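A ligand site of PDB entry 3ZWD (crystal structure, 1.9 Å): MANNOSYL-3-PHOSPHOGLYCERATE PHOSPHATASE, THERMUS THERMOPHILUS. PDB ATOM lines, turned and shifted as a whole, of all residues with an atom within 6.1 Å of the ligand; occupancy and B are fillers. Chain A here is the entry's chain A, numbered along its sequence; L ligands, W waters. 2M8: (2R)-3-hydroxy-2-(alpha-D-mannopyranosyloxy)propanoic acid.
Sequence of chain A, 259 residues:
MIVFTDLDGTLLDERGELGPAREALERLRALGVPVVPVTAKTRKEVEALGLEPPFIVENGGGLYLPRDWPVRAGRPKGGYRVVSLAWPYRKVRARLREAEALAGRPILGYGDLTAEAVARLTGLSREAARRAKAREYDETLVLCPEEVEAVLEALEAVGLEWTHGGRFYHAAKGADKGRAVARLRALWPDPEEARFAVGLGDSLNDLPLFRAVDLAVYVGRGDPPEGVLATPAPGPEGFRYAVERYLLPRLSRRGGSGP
O4 of the ligand sits at hydrogen-bond distance from OE2 of Glu 45 (2.5 Å).
The backbone carbonyl oxygen (O) of Gly 165 is in hydrogen-bond range of an oxygen (O13) of the ligand.
An oxygen (O1A) of the ligand sits at hydrogen-bond distance from a ring nitrogen (NE2) of His 170 (2.7 Å).
The side-chain hydroxyl (OG1) of Thr 140 lies within hydrogen-bond range of an oxygen (O2) of the ligand, 2.8 Å away.
O1B of the ligand is in hydrogen-bond range of N of Arg 167.
The guanidinium group of Arg 167 sits at hydrogen-bond distance from an oxygen (O6) of the ligand (2.9 Å).
NH1 of Arg 135 is in hydrogen-bond range of O3 of the ligand (2.8 Å).
The side-chain amino group of Lys 41 is in hydrogen-bond range of an oxygen (O4) of the ligand (2.9 Å).
OH of Tyr 110 sits close to O2 of the ligand, 2.9 Å away.
An oxygen (O1B) of the ligand is in hydrogen-bond range of the backbone NH of Phe 168 (3.5 Å).
Asp 8 touches the ligand.
Ala 40 touches the ligand (CB to O13, 3.5 Å).
CB of Thr 122 touches C6 of the ligand, at 3.95 Å.
Ala 132 touches the ligand.
Gly 166 touches the ligand.
Hydrophobic or aromatic side chains that line the ligand: Ala 40, Tyr 110, Ala 132, Phe 168 and His 170.
14 residues have an atom within 4 Å of the ligand: Asp 8, Ala 40, Lys 41, Glu 45, Tyr 110, Thr 122, Ala 132, Arg 135, Thr 140, Gly 165, Gly 166, Arg 167, Phe 168 and His 170.
The backbone NH (N) of Thr 42 lies within hydrogen-bond range of the side-chain carboxylate (OE1) of Glu 45 (2.9 Å).
ND1 of His 170 sits close to OG1 of Thr 140, at 3.4 Å.
The side-chain carboxylate of Asp 138 is in hydrogen-bond range of a ring nitrogen (ND1) of His 170.
The backbone carbonyl oxygen of Thr 122 lies within hydrogen-bond range of the guanidinium group of Arg 167, 2.6 Å away.
The backbone carbonyl oxygen (O) of Ala 132 sits at hydrogen-bond distance from the guanidinium group (NH1) of Arg 135, at 2.9 Å.
The guanidinium group (NH2) of Arg 135 is in salt-bridge range of the side-chain carboxylate (OD1) of Asp 138.
A ring nitrogen (ND1) of His 164 is in hydrogen-bond range of the backbone NH of Gly 166 (3.2 Å).
The side-chain hydroxyl of Thr 122 lies within hydrogen-bond range of the backbone NH of Leu 124, 3.0 Å away.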
ATOM      1  N   ASP A   6      -0.583  32.403  -3.824  1.00  0.00           N
ATOM      2  CA  ASP A   6       0.316  31.641  -2.962  1.00  0.00           C
ATOM      3  C   ASP A   6       1.235  32.609  -2.209  1.00  0.00           C
ATOM      4  O   ASP A   6       1.954  33.396  -2.825  1.00  0.00           O
ATOM      5  CB  ASP A   6       1.130  30.638  -3.774  1.00  0.00           C
ATOM      6  CG  ASP A   6       1.901  29.645  -2.894  1.00  0.00           C
ATOM      7  OD1 ASP A   6       1.700  29.650  -1.658  1.00  0.00           O
ATOM      8  OD2 ASP A   6       2.729  28.878  -3.441  1.00  0.00           O
ATOM      9  N   ASP A   8       4.070  32.022  -0.073  1.00  0.00           N
ATOM     10  CA  ASP A   8       5.327  31.491  -0.618  1.00  0.00           C
ATOM     11  C   ASP A   8       6.306  32.555  -1.106  1.00  0.00           C
ATOM     12  O   ASP A   8       7.084  33.104  -0.336  1.00  0.00           O
ATOM     13  CB  ASP A   8       4.997  30.523  -1.760  1.00  0.00           C
ATOM     14  CG  ASP A   8       6.127  29.541  -2.044  1.00  0.00           C
ATOM     15  OD1 ASP A   8       7.228  29.703  -1.470  1.00  0.00           O
ATOM     16  OD2 ASP A   8       5.909  28.611  -2.842  1.00  0.00           O
ATOM     17  N   ALA A  40       0.978  26.825   1.691  1.00  0.00           N
ATOM     18  CA  ALA A  40       1.450  25.678   2.466  1.00  0.00           C
ATOM     19  C   ALA A  40       1.407  25.942   3.987  1.00  0.00           C
ATOM     20  O   ALA A  40       1.455  25.005   4.803  1.00  0.00           O
ATOM     21  CB  ALA A  40       2.900  25.309   2.032  1.00  0.00           C
ATOM     22  N   LYS A  41       1.318  27.212   4.371  1.00  0.00           N
ATOM     23  CA  LYS A  41       1.413  27.594   5.782  1.00  0.00           C
ATOM     24  C   LYS A  41       0.193  27.144   6.614  1.00  0.00           C
ATOM     25  O   LYS A  41      -0.864  26.849   6.061  1.00  0.00           O
ATOM     26  CB  LYS A  41       1.640  29.106   5.931  1.00  0.00           C
ATOM     27  CG  LYS A  41       3.000  29.586   5.411  1.00  0.00           C
ATOM     28  CD  LYS A  41       3.136  31.095   5.526  1.00  0.00           C
ATOM     29  CE  LYS A  41       4.469  31.593   4.967  1.00  0.00           C
ATOM     30  NZ  LYS A  41       5.641  30.979   5.645  1.00  0.00           N
ATOM     31  N   THR A  42       0.360  27.079   7.929  1.00  0.00           N
ATOM     32  CA  THR A  42      -0.757  26.734   8.803  1.00  0.00           C
ATOM     33  C   THR A  42      -1.661  27.932   9.074  1.00  0.00           C
ATOM     34  O   THR A  42      -1.305  29.080   8.828  1.00  0.00           O
ATOM     35  CB  THR A  42      -0.260  26.196  10.173  1.00  0.00           C
ATOM     36  OG1 THR A  42       0.384  27.261  10.895  1.00  0.00           O
ATOM     37  CG2 THR A  42       0.718  25.040   9.983  1.00  0.00           C
ATOM     38  N   GLU A  45       0.057  30.330  11.333  1.00  0.00           N
ATOM     39  CA  GLU A  45       0.973  31.203  10.608  1.00  0.00           C
ATOM     40  C   GLU A  45       0.243  32.370   9.926  1.00  0.00           C
ATOM     41  O   GLU A  45       0.647  33.518  10.057  1.00  0.00           O
ATOM     42  CB  GLU A  45       1.796  30.406   9.589  1.00  0.00           C
ATOM     43  CG  GLU A  45       2.834  29.449  10.214  1.00  0.00           C
ATOM     44  CD  GLU A  45       3.653  28.733   9.159  1.00  0.00           C
ATOM     45  OE1 GLU A  45       3.116  27.775   8.530  1.00  0.00           O
ATOM     46  OE2 GLU A  45       4.820  29.125   8.927  1.00  0.00           O
ATOM     47  N   ASN A  59      -1.606  23.646   1.920  1.00  0.00           N
ATOM     48  CA  ASN A  59      -1.658  23.114   0.557  1.00  0.00           C
ATOM     49  C   ASN A  59      -3.057  22.704   0.129  1.00  0.00           C
ATOM     50  O   ASN A  59      -3.217  21.869  -0.740  1.00  0.00           O
ATOM     51  CB  ASN A  59      -0.708  21.908   0.414  1.00  0.00           C
ATOM     52  CG  ASN A  59       0.753  22.326   0.323  1.00  0.00           C
ATOM     53  OD1 ASN A  59       1.066  23.385  -0.208  1.00  0.00           O
ATOM     54  ND2 ASN A  59       1.649  21.473   0.827  1.00  0.00           N
ATOM     55  N   TYR A 110       8.384  17.878  10.523  1.00  0.00           N
ATOM     56  CA  TYR A 110       8.282  18.881  11.584  1.00  0.00           C
ATOM     57  C   TYR A 110       7.815  18.285  12.898  1.00  0.00           C
ATOM     58  O   TYR A 110       8.217  18.748  13.959  1.00  0.00           O
ATOM     59  CB  TYR A 110       7.305  20.000  11.202  1.00  0.00           C
ATOM     60  CG  TYR A 110       7.818  21.032  10.228  1.00  0.00           C
ATOM     61  CD1 TYR A 110       9.058  20.918   9.601  1.00  0.00           C
ATOM     62  CD2 TYR A 110       7.043  22.161   9.947  1.00  0.00           C
ATOM     63  CE1 TYR A 110       9.509  21.901   8.704  1.00  0.00           C
ATOM     64  CE2 TYR A 110       7.470  23.136   9.082  1.00  0.00           C
ATOM     65  CZ  TYR A 110       8.694  22.996   8.446  1.00  0.00           C
ATOM     66  OH  TYR A 110       9.063  23.990   7.559  1.00  0.00           O
ATOM     67  N   THR A 122      14.345  26.569   8.398  1.00  0.00           N
ATOM     68  CA  THR A 122      13.449  27.368   7.558  1.00  0.00           C
ATOM     69  C   THR A 122      13.858  28.826   7.475  1.00  0.00           C
ATOM     70  O   THR A 122      13.445  29.546   6.559  1.00  0.00           O
ATOM     71  CB  THR A 122      12.015  27.362   8.101  1.00  0.00           C
ATOM     72  OG1 THR A 122      11.998  27.941   9.425  1.00  0.00           O
ATOM     73  CG2 THR A 122      11.448  25.942   8.134  1.00  0.00           C
ATOM     74  N   LEU A 124      12.922  30.806   9.795  1.00  0.00           N
ATOM     75  CA  LEU A 124      11.890  31.460  10.593  1.00  0.00           C
ATOM     76  C   LEU A 124      12.416  31.734  12.000  1.00  0.00           C
ATOM     77  O   LEU A 124      13.435  31.171  12.399  1.00  0.00           O
ATOM     78  CB  LEU A 124      10.637  30.583  10.707  1.00  0.00           C
ATOM     79  CG  LEU A 124       9.834  30.182   9.462  1.00  0.00           C
ATOM     80  CD1 LEU A 124       8.811  29.121   9.844  1.00  0.00           C
ATOM     81  CD2 LEU A 124       9.169  31.395   8.802  1.00  0.00           C
ATOM     82  N   ALA A 132       4.433  27.224  12.555  1.00  0.00           N
ATOM     83  CA  ALA A 132       4.592  26.316  11.423  1.00  0.00           C
ATOM     84  C   ALA A 132       4.475  24.841  11.854  1.00  0.00           C
ATOM     85  O   ALA A 132       4.174  23.956  11.036  1.00  0.00           O
ATOM     86  CB  ALA A 132       5.925  26.564  10.700  1.00  0.00           C
ATOM     87  N   ARG A 135       0.392  21.984  12.809  1.00  0.00           N
ATOM     88  CA  ARG A 135      -0.177  21.519  11.546  1.00  0.00           C
ATOM     89  C   ARG A 135      -1.383  20.624  11.767  1.00  0.00           C
ATOM     90  O   ARG A 135      -1.358  19.707  12.609  1.00  0.00           O
ATOM     91  CB  ARG A 135       0.898  20.784  10.712  1.00  0.00           C
ATOM     92  CG  ARG A 135       2.218  21.572  10.636  1.00  0.00           C
ATOM     93  CD  ARG A 135       3.171  21.052   9.563  1.00  0.00           C
ATOM     94  NE  ARG A 135       2.724  21.393   8.208  1.00  0.00           N
ATOM     95  CZ  ARG A 135       2.896  22.575   7.622  1.00  0.00           C
ATOM     96  NH1 ARG A 135       3.480  23.570   8.264  1.00  0.00           N
ATOM     97  NH2 ARG A 135       2.473  22.765   6.363  1.00  0.00           N
ATOM     98  N   ASP A 138      -1.224  18.535   7.041  1.00  0.00           N
ATOM     99  CA  ASP A 138      -0.134  18.284   6.115  1.00  0.00           C
ATOM    100  C   ASP A 138       1.154  18.236   6.936  1.00  0.00           C
ATOM    101  O   ASP A 138       1.324  19.010   7.864  1.00  0.00           O
ATOM    102  CB  ASP A 138      -0.105  19.439   5.116  1.00  0.00           C
ATOM    103  CG  ASP A 138       1.202  19.560   4.362  1.00  0.00           C
ATOM    104  OD1 ASP A 138       2.188  20.113   4.925  1.00  0.00           O
ATOM    105  OD2 ASP A 138       1.254  19.125   3.192  1.00  0.00           O
ATOM    106  N   THR A 140       5.277  18.673   6.906  1.00  0.00           N
ATOM    107  CA  THR A 140       6.447  19.106   6.153  1.00  0.00           C
ATOM    108  C   THR A 140       7.609  18.155   6.445  1.00  0.00           C
ATOM    109  O   THR A 140       7.987  17.967   7.612  1.00  0.00           O
ATOM    110  CB  THR A 140       6.819  20.558   6.501  1.00  0.00           C
ATOM    111  OG1 THR A 140       5.685  21.403   6.241  1.00  0.00           O
ATOM    112  CG2 THR A 140       8.013  21.033   5.672  1.00  0.00           C
ATOM    113  N   HIS A 164       5.780  19.285  -3.605  1.00  0.00           N
ATOM    114  CA  HIS A 164       6.921  20.126  -3.257  1.00  0.00           C
ATOM    115  C   HIS A 164       6.481  21.586  -3.115  1.00  0.00           C
ATOM    116  O   HIS A 164       5.811  22.132  -4.002  1.00  0.00           O
ATOM    117  CB  HIS A 164       8.054  20.003  -4.278  1.00  0.00           C
ATOM    118  CG  HIS A 164       9.392  20.446  -3.758  1.00  0.00           C
ATOM    119  ND1 HIS A 164       9.759  21.767  -3.675  1.00  0.00           N
ATOM    120  CD2 HIS A 164      10.444  19.739  -3.275  1.00  0.00           C
ATOM    121  CE1 HIS A 164      10.980  21.859  -3.170  1.00  0.00           C
ATOM    122  NE2 HIS A 164      11.416  20.635  -2.921  1.00  0.00           N
ATOM    123  N   GLY A 165       6.845  22.208  -1.995  1.00  0.00           N
ATOM    124  CA  GLY A 165       6.331  23.532  -1.671  1.00  0.00           C
ATOM    125  C   GLY A 165       7.243  24.689  -2.026  1.00  0.00           C
ATOM    126  O   GLY A 165       6.834  25.854  -1.950  1.00  0.00           O
ATOM    127  N   GLY A 166       8.472  24.380  -2.411  1.00  0.00           N
ATOM    128  CA  GLY A 166       9.440  25.412  -2.694  1.00  0.00           C
ATOM    129  C   GLY A 166      10.806  25.036  -2.154  1.00  0.00           C
ATOM    130  O   GLY A 166      11.810  25.199  -2.843  1.00  0.00           O
ATOM    131  N   ARG A 167      10.839  24.545  -0.920  1.00  0.00           N
ATOM    132  CA  ARG A 167      12.078  24.046  -0.319  1.00  0.00           C
ATOM    133  C   ARG A 167      11.910  22.655   0.297  1.00  0.00           C
ATOM    134  O   ARG A 167      12.850  21.879   0.337  1.00  0.00           O
ATOM    135  CB  ARG A 167      12.604  25.030   0.722  1.00  0.00           C
ATOM    136  CG  ARG A 167      13.009  26.376   0.139  1.00  0.00           C
ATOM    137  CD  ARG A 167      13.745  27.235   1.160  1.00  0.00           C
ATOM    138  NE  ARG A 167      12.895  27.569   2.305  1.00  0.00           N
ATOM    139  CZ  ARG A 167      13.357  28.043   3.460  1.00  0.00           C
ATOM    140  NH1 ARG A 167      14.660  28.226   3.632  1.00  0.00           N
ATOM    141  NH2 ARG A 167      12.511  28.309   4.441  1.00  0.00           N
ATOM    142  N   PHE A 168      10.699  22.332   0.766  1.00  0.00           N
ATOM    143  CA  PHE A 168      10.454  21.047   1.399  1.00  0.00           C
ATOM    144  C   PHE A 168       9.433  20.192   0.682  1.00  0.00           C
ATOM    145  O   PHE A 168       8.529  20.701   0.020  1.00  0.00           O
ATOM    146  CB  PHE A 168       9.948  21.236   2.820  1.00  0.00           C
ATOM    147  CG  PHE A 168      10.867  22.061   3.674  1.00  0.00           C
ATOM    148  CD1 PHE A 168      11.947  21.478   4.289  1.00  0.00           C
ATOM    149  CD2 PHE A 168      10.627  23.413   3.851  1.00  0.00           C
ATOM    150  CE1 PHE A 168      12.795  22.226   5.075  1.00  0.00           C
ATOM    151  CE2 PHE A 168      11.479  24.172   4.631  1.00  0.00           C
ATOM    152  CZ  PHE A 168      12.562  23.573   5.246  1.00  0.00           C
ATOM    153  N   TYR A 169       9.563  18.877   0.832  1.00  0.00           N
ATOM    154  CA  TYR A 169       8.511  17.967   0.432  1.00  0.00           C
ATOM    155  C   TYR A 169       7.470  17.960   1.515  1.00  0.00           C
ATOM    156  O   TYR A 169       7.770  18.164   2.705  1.00  0.00           O
ATOM    157  CB  TYR A 169       9.060  16.563   0.219  1.00  0.00           C
ATOM    158  CG  TYR A 169       9.880  16.450  -1.052  1.00  0.00           C
ATOM    159  CD1 TYR A 169       9.255  16.252  -2.280  1.00  0.00           C
ATOM    160  CD2 TYR A 169      11.259  16.560  -1.018  1.00  0.00           C
ATOM    161  CE1 TYR A 169       9.989  16.151  -3.435  1.00  0.00           C
ATOM    162  CE2 TYR A 169      12.007  16.461  -2.178  1.00  0.00           C
ATOM    163  CZ  TYR A 169      11.360  16.255  -3.388  1.00  0.00           C
ATOM    164  OH  TYR A 169      12.102  16.161  -4.541  1.00  0.00           O
ATOM    165  N   HIS A 170       6.222  17.738   1.107  1.00  0.00           N
ATOM    166  CA  HIS A 170       5.114  17.635   2.032  1.00  0.00           C
ATOM    167  C   HIS A 170       4.397  16.314   1.829  1.00  0.00           C
ATOM    168  O   HIS A 170       4.365  15.785   0.706  1.00  0.00           O
ATOM    169  CB  HIS A 170       4.119  18.778   1.820  1.00  0.00           C
ATOM    170  CG  HIS A 170       4.659  20.128   2.183  1.00  0.00           C
ATOM    171  ND1 HIS A 170       4.204  20.843   3.261  1.00  0.00           N
ATOM    172  CD2 HIS A 170       5.608  20.892   1.592  1.00  0.00           C
ATOM    173  CE1 HIS A 170       4.854  21.992   3.333  1.00  0.00           C
ATOM    174  NE2 HIS A 170       5.714  22.043   2.332  1.00  0.00           N
ATOM    175  N   LYS A 177      -4.265  22.346  -3.728  1.00  0.00           N
ATOM    176  CA  LYS A 177      -4.671  23.752  -3.859  1.00  0.00           C
ATOM    177  C   LYS A 177      -5.824  23.999  -4.827  1.00  0.00           C
ATOM    178  O   LYS A 177      -6.700  24.823  -4.543  1.00  0.00           O
ATOM    179  CB  LYS A 177      -3.484  24.666  -4.176  1.00  0.00           C
ATOM    180  CG  LYS A 177      -2.447  24.698  -3.018  1.00  0.00           C
ATOM    181  CD  LYS A 177      -1.422  25.805  -3.229  1.00  0.00           C
ATOM    182  CE  LYS A 177      -0.410  25.821  -2.083  1.00  0.00           C
ATOM    183  NZ  LYS A 177       0.555  26.962  -2.202  1.00  0.00           N
HETATM  184  C1  2M8 L   1       6.826  25.062   4.462  1.00  0.00           C
HETATM  185  O1  2M8 L   1       6.263  25.653   3.290  1.00  0.00           O
HETATM  186  C22 2M8 L   1       7.260  26.179   2.413  1.00  0.00           C
HETATM  187  C23 2M8 L   1       6.585  27.107   1.403  1.00  0.00           C
HETATM  188  O13 2M8 L   1       5.881  26.308   0.444  1.00  0.00           O
HETATM  189  C21 2M8 L   1       7.986  25.065   1.703  1.00  0.00           C
HETATM  190  O1A 2M8 L   1       7.447  23.950   1.610  1.00  0.00           O
HETATM  191  O1B 2M8 L   1       9.021  25.362   1.060  1.00  0.00           O
HETATM  192  C2  2M8 L   1       5.726  24.876   5.509  1.00  0.00           C
HETATM  193  O2  2M8 L   1       6.297  24.102   6.583  1.00  0.00           O
HETATM  194  C3  2M8 L   1       5.245  26.227   6.017  1.00  0.00           C
HETATM  195  O3  2M8 L   1       4.362  26.012   7.130  1.00  0.00           O
HETATM  196  C4  2M8 L   1       6.439  27.051   6.509  1.00  0.00           C
HETATM  197  O4  2M8 L   1       6.060  28.391   6.866  1.00  0.00           O
HETATM  198  C5  2M8 L   1       7.494  27.159   5.419  1.00  0.00           C
HETATM  199  C6  2M8 L   1       8.736  27.886   5.954  1.00  0.00           C
HETATM  200  O6  2M8 L   1       9.606  28.211   4.867  1.00  0.00           O
HETATM  201  O5  2M8 L   1       7.887  25.860   4.978  1.00  0.00           O
HETATM  202  O   HOH W   1       9.775  27.941   0.601  1.00  0.00           O
